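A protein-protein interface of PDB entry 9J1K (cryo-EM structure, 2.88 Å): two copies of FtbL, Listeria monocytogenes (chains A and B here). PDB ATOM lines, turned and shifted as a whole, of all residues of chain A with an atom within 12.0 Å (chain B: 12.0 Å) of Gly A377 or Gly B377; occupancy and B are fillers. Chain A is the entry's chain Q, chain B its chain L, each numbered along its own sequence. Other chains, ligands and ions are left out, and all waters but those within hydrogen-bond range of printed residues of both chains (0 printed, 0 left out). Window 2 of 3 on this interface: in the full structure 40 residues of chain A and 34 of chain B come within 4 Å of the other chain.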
ATOM      1  N   ILE A 367      16.723   6.513   8.884  1.00  0.00           N
ATOM      2  CA  ILE A 367      17.852   7.286   9.394  1.00  0.00           C
ATOM      3  C   ILE A 367      17.740   8.737   8.952  1.00  0.00           C
ATOM      4  O   ILE A 367      17.882   9.662   9.757  1.00  0.00           O
ATOM      5  CB  ILE A 367      19.186   6.665   8.940  1.00  0.00           C
ATOM      6  CG1 ILE A 367      19.505   5.406   9.742  1.00  0.00           C
ATOM      7  CG2 ILE A 367      20.319   7.674   9.066  1.00  0.00           C
ATOM      8  CD1 ILE A 367      20.621   4.592   9.138  1.00  0.00           C
ATOM      9  N   LEU A 368      17.478   8.957   7.661  1.00  0.00           N
ATOM     10  CA  LEU A 368      17.358  10.317   7.143  1.00  0.00           C
ATOM     11  C   LEU A 368      16.179  11.050   7.770  1.00  0.00           C
ATOM     12  O   LEU A 368      16.296  12.227   8.138  1.00  0.00           O
ATOM     13  CB  LEU A 368      17.218  10.292   5.621  1.00  0.00           C
ATOM     14  CG  LEU A 368      18.445   9.864   4.815  1.00  0.00           C
ATOM     15  CD1 LEU A 368      18.077   9.657   3.354  1.00  0.00           C
ATOM     16  CD2 LEU A 368      19.560  10.889   4.951  1.00  0.00           C
ATOM     17  N   THR A 369      15.033  10.376   7.898  1.00  0.00           N
ATOM     18  CA  THR A 369      13.855  11.035   8.460  1.00  0.00           C
ATOM     19  C   THR A 369      14.108  11.483   9.897  1.00  0.00           C
ATOM     20  O   THR A 369      13.837  12.635  10.261  1.00  0.00           O
ATOM     21  CB  THR A 369      12.640  10.108   8.397  1.00  0.00           C
ATOM     22  OG1 THR A 369      12.925   8.893   9.099  1.00  0.00           O
ATOM     23  CG2 THR A 369      12.283   9.790   6.953  1.00  0.00           C
ATOM     24  N   GLU A 370      14.651  10.595  10.726  1.00  0.00           N
ATOM     25  CA  GLU A 370      14.899  10.964  12.111  1.00  0.00           C
ATOM     26  C   GLU A 370      16.107  11.877  12.283  1.00  0.00           C
ATOM     27  O   GLU A 370      16.166  12.613  13.271  1.00  0.00           O
ATOM     28  CB  GLU A 370      15.050   9.713  12.977  1.00  0.00           C
ATOM     29  CG  GLU A 370      13.713   9.119  13.400  1.00  0.00           C
ATOM     30  CD  GLU A 370      13.565   7.662  13.017  1.00  0.00           C
ATOM     31  OE1 GLU A 370      14.557   7.060  12.558  1.00  0.00           O
ATOM     32  OE2 GLU A 370      12.451   7.121  13.169  1.00  0.00           O
ATOM     33  N   VAL A 371      17.047  11.894  11.335  1.00  0.00           N
ATOM     34  CA  VAL A 371      18.107  12.896  11.373  1.00  0.00           C
ATOM     35  C   VAL A 371      17.539  14.275  11.059  1.00  0.00           C
ATOM     36  O   VAL A 371      17.928  15.277  11.672  1.00  0.00           O
ATOM     37  CB  VAL A 371      19.244  12.505  10.410  1.00  0.00           C
ATOM     38  CG1 VAL A 371      20.039  13.730   9.980  1.00  0.00           C
ATOM     39  CG2 VAL A 371      20.162  11.483  11.066  1.00  0.00           C
ATOM     40  N   VAL A 372      16.604  14.347  10.109  1.00  0.00           N
ATOM     41  CA  VAL A 372      15.894  15.598   9.856  1.00  0.00           C
ATOM     42  C   VAL A 372      15.127  16.028  11.101  1.00  0.00           C
ATOM     43  O   VAL A 372      15.101  17.213  11.457  1.00  0.00           O
ATOM     44  CB  VAL A 372      14.965  15.448   8.637  1.00  0.00           C
ATOM     45  CG1 VAL A 372      13.959  16.589   8.581  1.00  0.00           C
ATOM     46  CG2 VAL A 372      15.781  15.391   7.354  1.00  0.00           C
ATOM     47  N   GLY A 373      14.497  15.071  11.784  1.00  0.00           N
ATOM     48  CA  GLY A 373      13.830  15.391  13.039  1.00  0.00           C
ATOM     49  C   GLY A 373      14.784  15.918  14.098  1.00  0.00           C
ATOM     50  O   GLY A 373      14.460  16.857  14.829  1.00  0.00           O
ATOM     51  N   VAL A 374      15.971  15.315  14.198  1.00  0.00           N
ATOM     52  CA  VAL A 374      16.975  15.777  15.155  1.00  0.00           C
ATOM     53  C   VAL A 374      17.416  17.197  14.821  1.00  0.00           C
ATOM     54  O   VAL A 374      17.561  18.044  15.711  1.00  0.00           O
ATOM     55  CB  VAL A 374      18.168  14.802  15.185  1.00  0.00           C
ATOM     56  CG1 VAL A 374      19.444  15.516  15.606  1.00  0.00           C
ATOM     57  CG2 VAL A 374      17.875  13.636  16.118  1.00  0.00           C
ATOM     58  N   VAL A 375      17.636  17.477  13.533  1.00  0.00           N
ATOM     59  CA  VAL A 375      17.974  18.834  13.109  1.00  0.00           C
ATOM     60  C   VAL A 375      16.860  19.799  13.487  1.00  0.00           C
ATOM     61  O   VAL A 375      17.115  20.925  13.931  1.00  0.00           O
ATOM     62  CB  VAL A 375      18.266  18.864  11.595  1.00  0.00           C
ATOM     63  CG1 VAL A 375      18.440  20.297  11.114  1.00  0.00           C
ATOM     64  CG2 VAL A 375      19.506  18.043  11.280  1.00  0.00           C
ATOM     65  N   ASP A 376      15.605  19.373  13.316  1.00  0.00           N
ATOM     66  CA  ASP A 376      14.478  20.168  13.795  1.00  0.00           C
ATOM     67  C   ASP A 376      14.560  20.397  15.298  1.00  0.00           C
ATOM     68  O   ASP A 376      14.128  21.444  15.792  1.00  0.00           O
ATOM     69  CB  ASP A 376      13.159  19.484  13.435  1.00  0.00           C
ATOM     70  CG  ASP A 376      12.864  19.527  11.950  1.00  0.00           C
ATOM     71  OD1 ASP A 376      13.517  20.316  11.234  1.00  0.00           O
ATOM     72  OD2 ASP A 376      11.980  18.771  11.497  1.00  0.00           O
ATOM     73  N   GLY A 377      15.102  19.427  16.037  1.00  0.00           N
ATOM     74  CA  GLY A 377      15.312  19.625  17.462  1.00  0.00           C
ATOM     75  C   GLY A 377      16.270  20.764  17.758  1.00  0.00           C
ATOM     76  O   GLY A 377      16.088  21.505  18.727  1.00  0.00           O
ATOM     77  N   ASP A 378      17.299  20.917  16.931  1.00  0.00           N
ATOM     78  CA  ASP A 378      18.246  22.016  17.080  1.00  0.00           C
ATOM     79  C   ASP A 378      17.629  23.332  16.616  1.00  0.00           C
ATOM     80  O   ASP A 378      17.311  24.201  17.428  1.00  0.00           O
ATOM     81  CB  ASP A 378      19.529  21.733  16.294  1.00  0.00           C
ATOM     82  CG  ASP A 378      20.415  20.708  16.974  1.00  0.00           C
ATOM     83  OD1 ASP A 378      20.178  20.413  18.163  1.00  0.00           O
ATOM     84  OD2 ASP A 378      21.348  20.197  16.319  1.00  0.00           O
ATOM     85  N   LEU B 368      12.329   3.736  17.631  1.00  0.00           N
ATOM     86  CA  LEU B 368      11.627   4.356  18.750  1.00  0.00           C
ATOM     87  C   LEU B 368      12.545   5.290  19.528  1.00  0.00           C
ATOM     88  O   LEU B 368      12.128   6.377  19.943  1.00  0.00           O
ATOM     89  CB  LEU B 368      11.051   3.281  19.672  1.00  0.00           C
ATOM     90  CG  LEU B 368       9.942   2.401  19.095  1.00  0.00           C
ATOM     91  CD1 LEU B 368       9.630   1.247  20.036  1.00  0.00           C
ATOM     92  CD2 LEU B 368       8.693   3.224  18.821  1.00  0.00           C
ATOM     93  N   THR B 369      13.797   4.877  19.747  1.00  0.00           N
ATOM     94  CA  THR B 369      14.746   5.744  20.442  1.00  0.00           C
ATOM     95  C   THR B 369      14.985   7.034  19.663  1.00  0.00           C
ATOM     96  O   THR B 369      15.022   8.127  20.243  1.00  0.00           O
ATOM     97  CB  THR B 369      16.071   5.016  20.679  1.00  0.00           C
ATOM     98  OG1 THR B 369      16.689   4.715  19.422  1.00  0.00           O
ATOM     99  CG2 THR B 369      15.850   3.732  21.465  1.00  0.00           C
ATOM    100  N   GLU B 370      15.153   6.924  18.342  1.00  0.00           N
ATOM    101  CA  GLU B 370      15.343   8.111  17.512  1.00  0.00           C
ATOM    102  C   GLU B 370      14.132   9.030  17.587  1.00  0.00           C
ATOM    103  O   GLU B 370      14.278  10.254  17.679  1.00  0.00           O
ATOM    104  CB  GLU B 370      15.607   7.717  16.058  1.00  0.00           C
ATOM    105  CG  GLU B 370      16.705   6.694  15.849  1.00  0.00           C
ATOM    106  CD  GLU B 370      17.152   6.603  14.404  1.00  0.00           C
ATOM    107  OE1 GLU B 370      17.206   7.646  13.724  1.00  0.00           O
ATOM    108  OE2 GLU B 370      17.426   5.476  13.939  1.00  0.00           O
ATOM    109  N   VAL B 371      12.926   8.458  17.540  1.00  0.00           N
ATOM    110  CA  VAL B 371      11.711   9.267  17.595  1.00  0.00           C
ATOM    111  C   VAL B 371      11.604   9.983  18.938  1.00  0.00           C
ATOM    112  O   VAL B 371      11.271  11.174  19.003  1.00  0.00           O
ATOM    113  CB  VAL B 371      10.476   8.392  17.318  1.00  0.00           C
ATOM    114  CG1 VAL B 371       9.205   9.090  17.779  1.00  0.00           C
ATOM    115  CG2 VAL B 371      10.393   8.047  15.838  1.00  0.00           C
ATOM    116  N   VAL B 372      11.884   9.266  20.030  1.00  0.00           N
ATOM    117  CA  VAL B 372      11.818   9.871  21.358  1.00  0.00           C
ATOM    118  C   VAL B 372      12.834  10.998  21.482  1.00  0.00           C
ATOM    119  O   VAL B 372      12.532  12.070  22.021  1.00  0.00           O
ATOM    120  CB  VAL B 372      12.023   8.798  22.445  1.00  0.00           C
ATOM    121  CG1 VAL B 372      12.225   9.447  23.806  1.00  0.00           C
ATOM    122  CG2 VAL B 372      10.836   7.850  22.482  1.00  0.00           C
ATOM    123  N   GLY B 373      14.051  10.780  20.982  1.00  0.00           N
ATOM    124  CA  GLY B 373      15.051  11.833  21.026  1.00  0.00           C
ATOM    125  C   GLY B 373      14.684  13.032  20.172  1.00  0.00           C
ATOM    126  O   GLY B 373      14.966  14.176  20.541  1.00  0.00           O
ATOM    127  N   VAL B 374      14.060  12.790  19.018  1.00  0.00           N
ATOM    128  CA  VAL B 374      13.610  13.885  18.163  1.00  0.00           C
ATOM    129  C   VAL B 374      12.554  14.713  18.882  1.00  0.00           C
ATOM    130  O   VAL B 374      12.583  15.949  18.860  1.00  0.00           O
ATOM    131  CB  VAL B 374      13.085  13.336  16.823  1.00  0.00           C
ATOM    132  CG1 VAL B 374      12.151  14.337  16.157  1.00  0.00           C
ATOM    133  CG2 VAL B 374      14.241  12.981  15.905  1.00  0.00           C
ATOM    134  N   VAL B 375      11.604  14.039  19.534  1.00  0.00           N
ATOM    135  CA  VAL B 375      10.572  14.749  20.287  1.00  0.00           C
ATOM    136  C   VAL B 375      11.194  15.540  21.431  1.00  0.00           C
ATOM    137  O   VAL B 375      10.815  16.690  21.689  1.00  0.00           O
ATOM    138  CB  VAL B 375       9.503  13.762  20.793  1.00  0.00           C
ATOM    139  CG1 VAL B 375       8.493  14.478  21.676  1.00  0.00           C
ATOM    140  CG2 VAL B 375       8.801  13.097  19.620  1.00  0.00           C
ATOM    141  N   ASP B 376      12.158  14.939  22.134  1.00  0.00           N
ATOM    142  CA  ASP B 376      12.809  15.629  23.244  1.00  0.00           C
ATOM    143  C   ASP B 376      13.570  16.860  22.766  1.00  0.00           C
ATOM    144  O   ASP B 376      13.565  17.901  23.433  1.00  0.00           O
ATOM    145  CB  ASP B 376      13.747  14.670  23.978  1.00  0.00           C
ATOM    146  CG  ASP B 376      13.001  13.593  24.738  1.00  0.00           C
ATOM    147  OD1 ASP B 376      11.769  13.718  24.895  1.00  0.00           O
ATOM    148  OD2 ASP B 376      13.647  12.618  25.176  1.00  0.00           O
ATOM    149  N   GLY B 377      14.239  16.757  21.616  1.00  0.00           N
ATOM    150  CA  GLY B 377      14.998  17.889  21.108  1.00  0.00           C
ATOM    151  C   GLY B 377      14.121  19.068  20.735  1.00  0.00           C
ATOM    152  O   GLY B 377      14.508  20.225  20.921  1.00  0.00           O
ATOM    153  N   ASP B 378      12.934  18.794  20.199  1.00  0.00           N
ATOM    154  CA  ASP B 378      12.002  19.846  19.808  1.00  0.00           C
ATOM    155  C   ASP B 378      11.528  20.648  21.016  1.00  0.00           C
ATOM    156  O   ASP B 378      11.294  21.853  20.921  1.00  0.00           O
ATOM    157  CB  ASP B 378      10.800  19.250  19.072  1.00  0.00           C
ATOM    158  CG  ASP B 378      11.110  18.909  17.627  1.00  0.00           C
ATOM    159  OD1 ASP B 378      12.121  19.415  17.099  1.00  0.00           O
ATOM    160  OD2 ASP B 378      10.341  18.135  17.020  1.00  0.00           O
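Glu B370 touches its own counterpart, Glu A370. Glu A370 touches Val B374, but with the chains exchanged Val A374 does not touch Glu B370 (5.2 Å). Gly A373 touches Val B374, but with the chains exchanged Val A374 does not touch Gly B373 (5.2 Å). Gly A377 touches Asp B378, but with the chains exchanged Asp A378 does not touch Gly B377 (4.9 Å). Of the 8 pairs that touch across the chains among the printed residues, 3 have their exchanged pair printed and touching as well.
Printed residues of chain B within 4 Å of Glu A370: Glu B370, Val B371 and Val B374. No residue of chain B comes within 4 Å of Val A375. Asp A376 touches just one residue of chain B: Asp B378 (3.1 Å). Gly A377 touches just these residues of chain B: Gly B377 and Asp B378. No residue of chain B comes within 4 Å of Asp A378. Leu B368 touches none of the printed residues of chain A. Printed residues of chain A within 4 Å of Val B371: Glu A370 (3.5 Å). No residue of chain A comes within 4 Å of Gly B373. Of the printed residues of chain A, Val B374 touches Glu A370, Gly A373 and Val A374. No residue of chain A comes within 4 Å of Val B375. Asp B376 touches none of the printed residues of chain A. Printed residues of chain A within 4 Å of Gly B377: Gly A377 (3.0 Å). Asp B378 touches just these residues of chain A: Asp A376 and Gly A377. The nearest residue of chain B that does not touch Gly A377 is Val B374 (4.8 Å). The nearest residue of chain A that does not touch Gly B377 is Asp A378 (4.9 Å). The nearest printed residue of chain A that does not touch Val B371 is Thr A369 (7.2 Å).
Of the 12 printed residues of chain A, 5 touch a printed residue of chain B. Hydrophobic or aromatic side chains of chain A that line the printed part of chain B: Val A374. Along chain A the printed residues that touch a printed residue of chain B span positions 370 to 377. Of the 11 printed residues of chain B, 5 touch a printed residue of chain A. Among the printed residues, 8 pairs touch across the chains.
The side-chain carboxylate of Asp B378 is in hydrogen-bond range of the backbone NH of Gly A377 (3.2 Å). The side-chain carboxylate (OE1) of Glu B370 sits close to the side-chain carboxylate (OE1) of Glu A370 (3.0 Å). O of Asp A376 lies close to OD1 of Asp B378 (3.1 Å). The backbone carbonyl oxygen (O) of Gly B377 sits close to the backbone carbonyl oxygen (O) of Gly A377 (3.0 Å).
Val B371 touches Glu A370. Val B374 touches Glu A370 (CG2 to O, 3.3 Å). Val B374 touches Gly A373 (CG2 to C, 3.5 Å). Val B374 touches Val A374 (CG2 to N, 3.4 Å).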
